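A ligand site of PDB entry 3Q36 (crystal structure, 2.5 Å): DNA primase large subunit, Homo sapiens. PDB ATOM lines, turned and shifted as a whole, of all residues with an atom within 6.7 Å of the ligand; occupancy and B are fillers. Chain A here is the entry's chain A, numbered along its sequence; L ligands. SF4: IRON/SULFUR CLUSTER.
Pro 20 touches the ligand (CB to S2, 3.6 Å). CD of Pro 120 touches S1 of the ligand (3.9 Å). CD2 of Phe 121 touches FE2 of the ligand, at 3.99 Å. Leu 176 touches the ligand. Pro 179 touches the ligand. Hydrophobic or aromatic side chains that line the ligand: Pro 20, Pro 120, Phe 121, Leu 176 and Pro 179. Of the 27 residues printed, 9 come within 4 Å of the ligand.
FE3 of the ligand is bound by SG of Cys 159 (2.2 Å). N of Cys 22 sits close to S1 of the ligand, 3.7 Å away. The side-chain sulfur (SG) of Cys 102 is bound to an iron atom (FE1) of the ligand. The side-chain sulfur of Cys 22 binds an iron atom (FE4) of the ligand. The side-chain sulfur (SG) of Cys 119 is bound to an iron atom (FE2) of the ligand (2.2 Å).
N of Phe 121 sits close to SG of Cys 119 (3.6 Å). N of Leu 176 sits at hydrogen-bond distance from OE1 of Gln 160 (2.8 Å). The side-chain sulfur of Cys 102 sits close to the backbone NH of His 178, at 3.4 Å. SG of Cys 119 lies close to N of Arg 122, at 3.7 Å. The backbone NH (N) of Cys 102 lies within hydrogen-bond range of the backbone carbonyl oxygen (O) of Asn 177, 3.1 Å away.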
ATOM      1  N   PRO A  20      22.205 -26.710  26.527  1.00  0.00           N
ATOM      2  CA  PRO A  20      23.561 -26.197  26.747  1.00  0.00           C
ATOM      3  C   PRO A  20      23.428 -25.070  27.795  1.00  0.00           C
ATOM      4  O   PRO A  20      22.306 -24.697  28.152  1.00  0.00           O
ATOM      5  CB  PRO A  20      23.980 -25.665  25.363  1.00  0.00           C
ATOM      6  CG  PRO A  20      22.669 -25.319  24.718  1.00  0.00           C
ATOM      7  CD  PRO A  20      21.731 -26.453  25.165  1.00  0.00           C
ATOM      8  N   PRO A  21      24.545 -24.541  28.315  1.00  0.00           N
ATOM      9  CA  PRO A  21      24.366 -23.481  29.314  1.00  0.00           C
ATOM     10  C   PRO A  21      23.532 -22.239  28.972  1.00  0.00           C
ATOM     11  O   PRO A  21      22.913 -21.656  29.848  1.00  0.00           O
ATOM     12  CB  PRO A  21      25.810 -23.133  29.728  1.00  0.00           C
ATOM     13  CG  PRO A  21      26.697 -23.906  28.782  1.00  0.00           C
ATOM     14  CD  PRO A  21      25.903 -25.090  28.351  1.00  0.00           C
ATOM     15  N   CYS A  22      23.469 -21.839  27.710  1.00  0.00           N
ATOM     16  CA  CYS A  22      22.667 -20.667  27.373  1.00  0.00           C
ATOM     17  C   CYS A  22      21.152 -20.936  27.508  1.00  0.00           C
ATOM     18  O   CYS A  22      20.389 -20.092  28.001  1.00  0.00           O
ATOM     19  CB  CYS A  22      22.937 -20.221  25.948  1.00  0.00           C
ATOM     20  SG  CYS A  22      22.598 -21.523  24.764  1.00  0.00           S
ATOM     21  N   MET A  23      20.715 -22.117  27.085  1.00  0.00           N
ATOM     22  CA  MET A  23      19.305 -22.447  27.161  1.00  0.00           C
ATOM     23  C   MET A  23      18.907 -22.831  28.588  1.00  0.00           C
ATOM     24  O   MET A  23      17.793 -22.558  29.011  1.00  0.00           O
ATOM     25  CB  MET A  23      18.975 -23.566  26.155  1.00  0.00           C
ATOM     26  CG  MET A  23      19.360 -23.210  24.705  1.00  0.00           C
ATOM     27  SD  MET A  23      18.842 -21.538  24.164  1.00  0.00           S
ATOM     28  CE  MET A  23      19.140 -21.595  22.412  1.00  0.00           C
ATOM     29  N   GLN A  43      15.599 -16.328  21.431  1.00  0.00           N
ATOM     30  CA  GLN A  43      16.602 -17.387  21.511  1.00  0.00           C
ATOM     31  C   GLN A  43      16.053 -18.695  22.094  1.00  0.00           C
ATOM     32  O   GLN A  43      16.222 -19.760  21.488  1.00  0.00           O
ATOM     33  CB  GLN A  43      17.790 -16.912  22.345  1.00  0.00           C
ATOM     34  CG  GLN A  43      18.882 -17.952  22.523  1.00  0.00           C
ATOM     35  CD  GLN A  43      20.116 -17.363  23.159  1.00  0.00           C
ATOM     36  OE1 GLN A  43      20.527 -16.250  22.822  1.00  0.00           O
ATOM     37  NE2 GLN A  43      20.734 -18.106  24.079  1.00  0.00           N
ATOM     38  N   SER A 101      22.159 -20.115  16.049  1.00  0.00           N
ATOM     39  CA  SER A 101      23.416 -20.850  16.093  1.00  0.00           C
ATOM     40  C   SER A 101      24.335 -20.191  17.129  1.00  0.00           C
ATOM     41  O   SER A 101      24.094 -19.060  17.569  1.00  0.00           O
ATOM     42  CB  SER A 101      24.104 -20.786  14.737  1.00  0.00           C
ATOM     43  OG  SER A 101      24.627 -19.482  14.533  1.00  0.00           O
ATOM     44  N   CYS A 102      25.394 -20.884  17.516  1.00  0.00           N
ATOM     45  CA  CYS A 102      26.310 -20.321  18.479  1.00  0.00           C
ATOM     46  C   CYS A 102      26.898 -18.978  18.020  1.00  0.00           C
ATOM     47  O   CYS A 102      26.966 -18.029  18.807  1.00  0.00           O
ATOM     48  CB  CYS A 102      27.434 -21.305  18.777  1.00  0.00           C
ATOM     49  SG  CYS A 102      26.889 -22.874  19.472  1.00  0.00           S
ATOM     50  N   LEU A 103      27.302 -18.869  16.757  1.00  0.00           N
ATOM     51  CA  LEU A 103      27.880 -17.621  16.294  1.00  0.00           C
ATOM     52  C   LEU A 103      26.907 -16.466  16.298  1.00  0.00           C
ATOM     53  O   LEU A 103      27.285 -15.326  16.572  1.00  0.00           O
ATOM     54  CB  LEU A 103      28.446 -17.751  14.887  1.00  0.00           C
ATOM     55  CG  LEU A 103      29.851 -18.298  14.790  1.00  0.00           C
ATOM     56  CD1 LEU A 103      30.192 -18.501  13.325  1.00  0.00           C
ATOM     57  CD2 LEU A 103      30.800 -17.335  15.463  1.00  0.00           C
ATOM     58  N   ILE A 105      24.357 -16.224  18.285  1.00  0.00           N
ATOM     59  CA  ILE A 105      24.178 -15.941  19.705  1.00  0.00           C
ATOM     60  C   ILE A 105      25.392 -15.213  20.245  1.00  0.00           C
ATOM     61  O   ILE A 105      25.259 -14.176  20.895  1.00  0.00           O
ATOM     62  CB  ILE A 105      23.937 -17.233  20.520  1.00  0.00           C
ATOM     63  CG1 ILE A 105      22.651 -17.920  20.022  1.00  0.00           C
ATOM     64  CG2 ILE A 105      23.893 -16.895  22.014  1.00  0.00           C
ATOM     65  CD1 ILE A 105      22.304 -19.284  20.658  1.00  0.00           C
ATOM     66  N   ILE A 106      26.573 -15.735  19.964  1.00  0.00           N
ATOM     67  CA  ILE A 106      27.795 -15.110  20.423  1.00  0.00           C
ATOM     68  C   ILE A 106      27.980 -13.712  19.878  1.00  0.00           C
ATOM     69  O   ILE A 106      28.321 -12.796  20.636  1.00  0.00           O
ATOM     70  CB  ILE A 106      29.037 -15.937  20.031  1.00  0.00           C
ATOM     71  CG1 ILE A 106      29.044 -17.235  20.823  1.00  0.00           C
ATOM     72  CG2 ILE A 106      30.317 -15.122  20.291  1.00  0.00           C
ATOM     73  CD1 ILE A 106      30.222 -18.100  20.496  1.00  0.00           C
ATOM     74  N   GLY A 118      22.035 -14.882  25.133  1.00  0.00           N
ATOM     75  CA  GLY A 118      23.435 -14.742  24.788  1.00  0.00           C
ATOM     76  C   GLY A 118      24.157 -16.033  25.093  1.00  0.00           C
ATOM     77  O   GLY A 118      23.525 -17.075  25.310  1.00  0.00           O
ATOM     78  N   CYS A 119      25.482 -15.978  25.089  1.00  0.00           N
ATOM     79  CA  CYS A 119      26.291 -17.149  25.390  1.00  0.00           C
ATOM     80  C   CYS A 119      26.946 -16.935  26.745  1.00  0.00           C
ATOM     81  O   CYS A 119      27.671 -15.976  26.960  1.00  0.00           O
ATOM     82  CB  CYS A 119      27.384 -17.347  24.345  1.00  0.00           C
ATOM     83  SG  CYS A 119      28.447 -18.785  24.656  1.00  0.00           S
ATOM     84  N   PRO A 120      26.663 -17.829  27.693  1.00  0.00           N
ATOM     85  CA  PRO A 120      27.263 -17.658  29.020  1.00  0.00           C
ATOM     86  C   PRO A 120      28.795 -17.547  28.934  1.00  0.00           C
ATOM     87  O   PRO A 120      29.404 -16.707  29.589  1.00  0.00           O
ATOM     88  CB  PRO A 120      26.811 -18.907  29.749  1.00  0.00           C
ATOM     89  CG  PRO A 120      25.513 -19.189  29.104  1.00  0.00           C
ATOM     90  CD  PRO A 120      25.724 -18.957  27.663  1.00  0.00           C
ATOM     91  N   PHE A 121      29.404 -18.387  28.109  1.00  0.00           N
ATOM     92  CA  PHE A 121      30.864 -18.362  27.949  1.00  0.00           C
ATOM     93  C   PHE A 121      31.391 -17.046  27.401  1.00  0.00           C
ATOM     94  O   PHE A 121      32.435 -16.581  27.807  1.00  0.00           O
ATOM     95  CB  PHE A 121      31.279 -19.497  27.052  1.00  0.00           C
ATOM     96  CG  PHE A 121      30.952 -20.828  27.619  1.00  0.00           C
ATOM     97  CD1 PHE A 121      31.693 -21.354  28.662  1.00  0.00           C
ATOM     98  CD2 PHE A 121      29.868 -21.550  27.134  1.00  0.00           C
ATOM     99  CE1 PHE A 121      31.345 -22.590  29.213  1.00  0.00           C
ATOM    100  CE2 PHE A 121      29.510 -22.779  27.691  1.00  0.00           C
ATOM    101  CZ  PHE A 121      30.247 -23.303  28.725  1.00  0.00           C
ATOM    102  N   ARG A 122      30.652 -16.446  26.472  1.00  0.00           N
ATOM    103  CA  ARG A 122      31.050 -15.178  25.871  1.00  0.00           C
ATOM    104  C   ARG A 122      30.510 -13.969  26.617  1.00  0.00           C
ATOM    105  O   ARG A 122      31.191 -12.957  26.729  1.00  0.00           O
ATOM    106  CB  ARG A 122      30.596 -15.142  24.410  1.00  0.00           C
ATOM    107  CG  ARG A 122      30.338 -13.735  23.842  1.00  0.00           C
ATOM    108  CD  ARG A 122      31.543 -13.130  23.067  1.00  0.00           C
ATOM    109  NE  ARG A 122      32.062 -11.924  23.715  1.00  0.00           N
ATOM    110  CZ  ARG A 122      31.338 -10.831  23.974  1.00  0.00           C
ATOM    111  NH1 ARG A 122      31.901  -9.788  24.591  1.00  0.00           N
ATOM    112  NH2 ARG A 122      30.058 -10.758  23.616  1.00  0.00           N
ATOM    113  N   TYR A 155      34.951 -20.164  22.957  1.00  0.00           N
ATOM    114  CA  TYR A 155      33.618 -20.379  23.535  1.00  0.00           C
ATOM    115  C   TYR A 155      32.986 -21.734  23.286  1.00  0.00           C
ATOM    116  O   TYR A 155      32.636 -22.427  24.228  1.00  0.00           O
ATOM    117  CB  TYR A 155      32.681 -19.266  23.068  1.00  0.00           C
ATOM    118  CG  TYR A 155      33.298 -17.898  23.259  1.00  0.00           C
ATOM    119  CD1 TYR A 155      33.716 -17.485  24.515  1.00  0.00           C
ATOM    120  CD2 TYR A 155      33.528 -17.040  22.181  1.00  0.00           C
ATOM    121  CE1 TYR A 155      34.346 -16.284  24.711  1.00  0.00           C
ATOM    122  CE2 TYR A 155      34.178 -15.810  22.363  1.00  0.00           C
ATOM    123  CZ  TYR A 155      34.576 -15.458  23.638  1.00  0.00           C
ATOM    124  OH  TYR A 155      35.268 -14.300  23.876  1.00  0.00           O
ATOM    125  N   GLN A 156      32.839 -22.100  22.018  1.00  0.00           N
ATOM    126  CA  GLN A 156      32.221 -23.378  21.689  1.00  0.00           C
ATOM    127  C   GLN A 156      32.984 -24.583  22.239  1.00  0.00           C
ATOM    128  O   GLN A 156      32.382 -25.631  22.530  1.00  0.00           O
ATOM    129  CB  GLN A 156      32.042 -23.526  20.179  1.00  0.00           C
ATOM    130  CG  GLN A 156      31.185 -22.436  19.537  1.00  0.00           C
ATOM    131  CD  GLN A 156      31.996 -21.213  19.109  1.00  0.00           C
ATOM    132  OE1 GLN A 156      32.747 -20.627  19.895  1.00  0.00           O
ATOM    133  NE2 GLN A 156      31.819 -20.809  17.844  1.00  0.00           N
ATOM    134  N   VAL A 157      34.294 -24.457  22.389  1.00  0.00           N
ATOM    135  CA  VAL A 157      35.071 -25.563  22.929  1.00  0.00           C
ATOM    136  C   VAL A 157      34.847 -25.681  24.445  1.00  0.00           C
ATOM    137  O   VAL A 157      34.816 -26.781  24.993  1.00  0.00           O
ATOM    138  CB  VAL A 157      36.562 -25.419  22.623  1.00  0.00           C
ATOM    139  CG1 VAL A 157      37.383 -26.315  23.532  1.00  0.00           C
ATOM    140  CG2 VAL A 157      36.799 -25.832  21.173  1.00  0.00           C
ATOM    141  N   ALA A 158      34.708 -24.545  25.118  1.00  0.00           N
ATOM    142  CA  ALA A 158      34.473 -24.554  26.537  1.00  0.00           C
ATOM    143  C   ALA A 158      33.115 -25.227  26.709  1.00  0.00           C
ATOM    144  O   ALA A 158      32.889 -26.018  27.620  1.00  0.00           O
ATOM    145  CB  ALA A 158      34.448 -23.141  27.071  1.00  0.00           C
ATOM    146  N   CYS A 159      32.205 -24.929  25.785  1.00  0.00           N
ATOM    147  CA  CYS A 159      30.898 -25.532  25.882  1.00  0.00           C
ATOM    148  C   CYS A 159      30.968 -27.033  25.656  1.00  0.00           C
ATOM    149  O   CYS A 159      30.187 -27.802  26.241  1.00  0.00           O
ATOM    150  CB  CYS A 159      29.916 -24.875  24.907  1.00  0.00           C
ATOM    151  SG  CYS A 159      28.194 -25.453  25.207  1.00  0.00           S
ATOM    152  N   GLN A 160      31.880 -27.480  24.798  1.00  0.00           N
ATOM    153  CA  GLN A 160      32.025 -28.921  24.551  1.00  0.00           C
ATOM    154  C   GLN A 160      32.579 -29.571  25.820  1.00  0.00           C
ATOM    155  O   GLN A 160      32.176 -30.676  26.211  1.00  0.00           O
ATOM    156  CB  GLN A 160      32.965 -29.184  23.384  1.00  0.00           C
ATOM    157  CG  GLN A 160      32.429 -28.660  22.047  1.00  0.00           C
ATOM    158  CD  GLN A 160      33.456 -28.765  20.929  1.00  0.00           C
ATOM    159  OE1 GLN A 160      33.260 -28.224  19.845  1.00  0.00           O
ATOM    160  NE2 GLN A 160      34.548 -29.462  21.199  1.00  0.00           N
ATOM    161  N   LEU A 176      31.129 -28.403  18.001  1.00  0.00           N
ATOM    162  CA  LEU A 176      29.955 -27.593  18.303  1.00  0.00           C
ATOM    163  C   LEU A 176      29.786 -26.273  17.566  1.00  0.00           C
ATOM    164  O   LEU A 176      30.732 -25.499  17.399  1.00  0.00           O
ATOM    165  CB  LEU A 176      29.918 -27.310  19.805  1.00  0.00           C
ATOM    166  CG  LEU A 176      28.634 -26.648  20.316  1.00  0.00           C
ATOM    167  CD1 LEU A 176      27.505 -27.670  20.437  1.00  0.00           C
ATOM    168  CD2 LEU A 176      28.930 -26.016  21.661  1.00  0.00           C
ATOM    169  N   ASN A 177      28.556 -26.039  17.107  1.00  0.00           N
ATOM    170  CA  ASN A 177      28.253 -24.771  16.443  1.00  0.00           C
ATOM    171  C   ASN A 177      26.760 -24.430  16.514  1.00  0.00           C
ATOM    172  O   ASN A 177      26.327 -23.415  15.968  1.00  0.00           O
ATOM    173  CB  ASN A 177      28.731 -24.766  14.991  1.00  0.00           C
ATOM    174  CG  ASN A 177      28.095 -25.837  14.166  1.00  0.00           C
ATOM    175  OD1 ASN A 177      28.786 -26.653  13.567  1.00  0.00           O
ATOM    176  ND2 ASN A 177      26.764 -25.850  14.127  1.00  0.00           N
ATOM    177  N   HIS A 178      25.984 -25.270  17.205  1.00  0.00           N
ATOM    178  CA  HIS A 178      24.542 -25.030  17.366  1.00  0.00           C
ATOM    179  C   HIS A 178      23.897 -25.648  18.623  1.00  0.00           C
ATOM    180  O   HIS A 178      23.942 -26.846  18.849  1.00  0.00           O
ATOM    181  CB  HIS A 178      23.790 -25.518  16.111  1.00  0.00           C
ATOM    182  CG  HIS A 178      22.512 -24.761  15.858  1.00  0.00           C
ATOM    183  ND1 HIS A 178      21.348 -24.995  16.568  1.00  0.00           N
ATOM    184  CD2 HIS A 178      22.235 -23.741  15.008  1.00  0.00           C
ATOM    185  CE1 HIS A 178      20.419 -24.151  16.165  1.00  0.00           C
ATOM    186  NE2 HIS A 178      20.926 -23.380  15.224  1.00  0.00           N
ATOM    187  N   PRO A 179      23.260 -24.799  19.440  1.00  0.00           N
ATOM    188  CA  PRO A 179      22.581 -25.196  20.678  1.00  0.00           C
ATOM    189  C   PRO A 179      21.710 -26.429  20.496  1.00  0.00           C
ATOM    190  O   PRO A 179      21.585 -27.251  21.388  1.00  0.00           O
ATOM    191  CB  PRO A 179      21.727 -23.971  21.033  1.00  0.00           C
ATOM    192  CG  PRO A 179      22.475 -22.836  20.471  1.00  0.00           C
ATOM    193  CD  PRO A 179      23.092 -23.349  19.186  1.00  0.00           C
ATOM    194  N   ASN A 180      21.093 -26.543  19.333  1.00  0.00           N
ATOM    195  CA  ASN A 180      20.228 -27.684  19.088  1.00  0.00           C
ATOM    196  C   ASN A 180      21.058 -28.940  18.794  1.00  0.00           C
ATOM    197  O   ASN A 180      20.612 -30.052  19.069  1.00  0.00           O
ATOM    198  CB  ASN A 180      19.241 -27.362  17.958  1.00  0.00           C
ATOM    199  CG  ASN A 180      18.212 -26.323  18.387  1.00  0.00           C
ATOM    200  OD1 ASN A 180      18.400 -25.126  18.190  1.00  0.00           O
ATOM    201  ND2 ASN A 180      17.122 -26.786  19.017  1.00  0.00           N
ATOM    202  N   PHE A 182      23.850 -29.537  20.294  1.00  0.00           N
ATOM    203  CA  PHE A 182      24.266 -29.926  21.645  1.00  0.00           C
ATOM    204  C   PHE A 182      23.151 -30.759  22.267  1.00  0.00           C
ATOM    205  O   PHE A 182      23.393 -31.783  22.886  1.00  0.00           O
ATOM    206  CB  PHE A 182      24.520 -28.648  22.483  1.00  0.00           C
ATOM    207  CG  PHE A 182      24.981 -28.884  23.911  1.00  0.00           C
ATOM    208  CD1 PHE A 182      26.201 -28.368  24.349  1.00  0.00           C
ATOM    209  CD2 PHE A 182      24.171 -29.550  24.831  1.00  0.00           C
ATOM    210  CE1 PHE A 182      26.617 -28.509  25.672  1.00  0.00           C
ATOM    211  CE2 PHE A 182      24.583 -29.704  26.164  1.00  0.00           C
ATOM    212  CZ  PHE A 182      25.804 -29.183  26.580  1.00  0.00           C
HETATM  213 FE1  SF4 L   1      26.900 -22.299  21.658  1.00  0.00          FE
HETATM  214 FE2  SF4 L   1      27.538 -20.683  24.009  1.00  0.00          FE
HETATM  215 FE3  SF4 L   1      27.279 -23.647  24.257  1.00  0.00          FE
HETATM  216 FE4  SF4 L   1      24.704 -21.921  23.737  1.00  0.00          FE
HETATM  217  S1  SF4 L   1      26.241 -21.994  25.195  1.00  0.00           S
HETATM  218  S2  SF4 L   1      25.594 -23.612  22.847  1.00  0.00           S
HETATM  219  S3  SF4 L   1      25.874 -20.596  22.577  1.00  0.00           S
HETATM  220  S4  SF4 L   1      28.470 -22.391  23.131  1.00  0.00           S
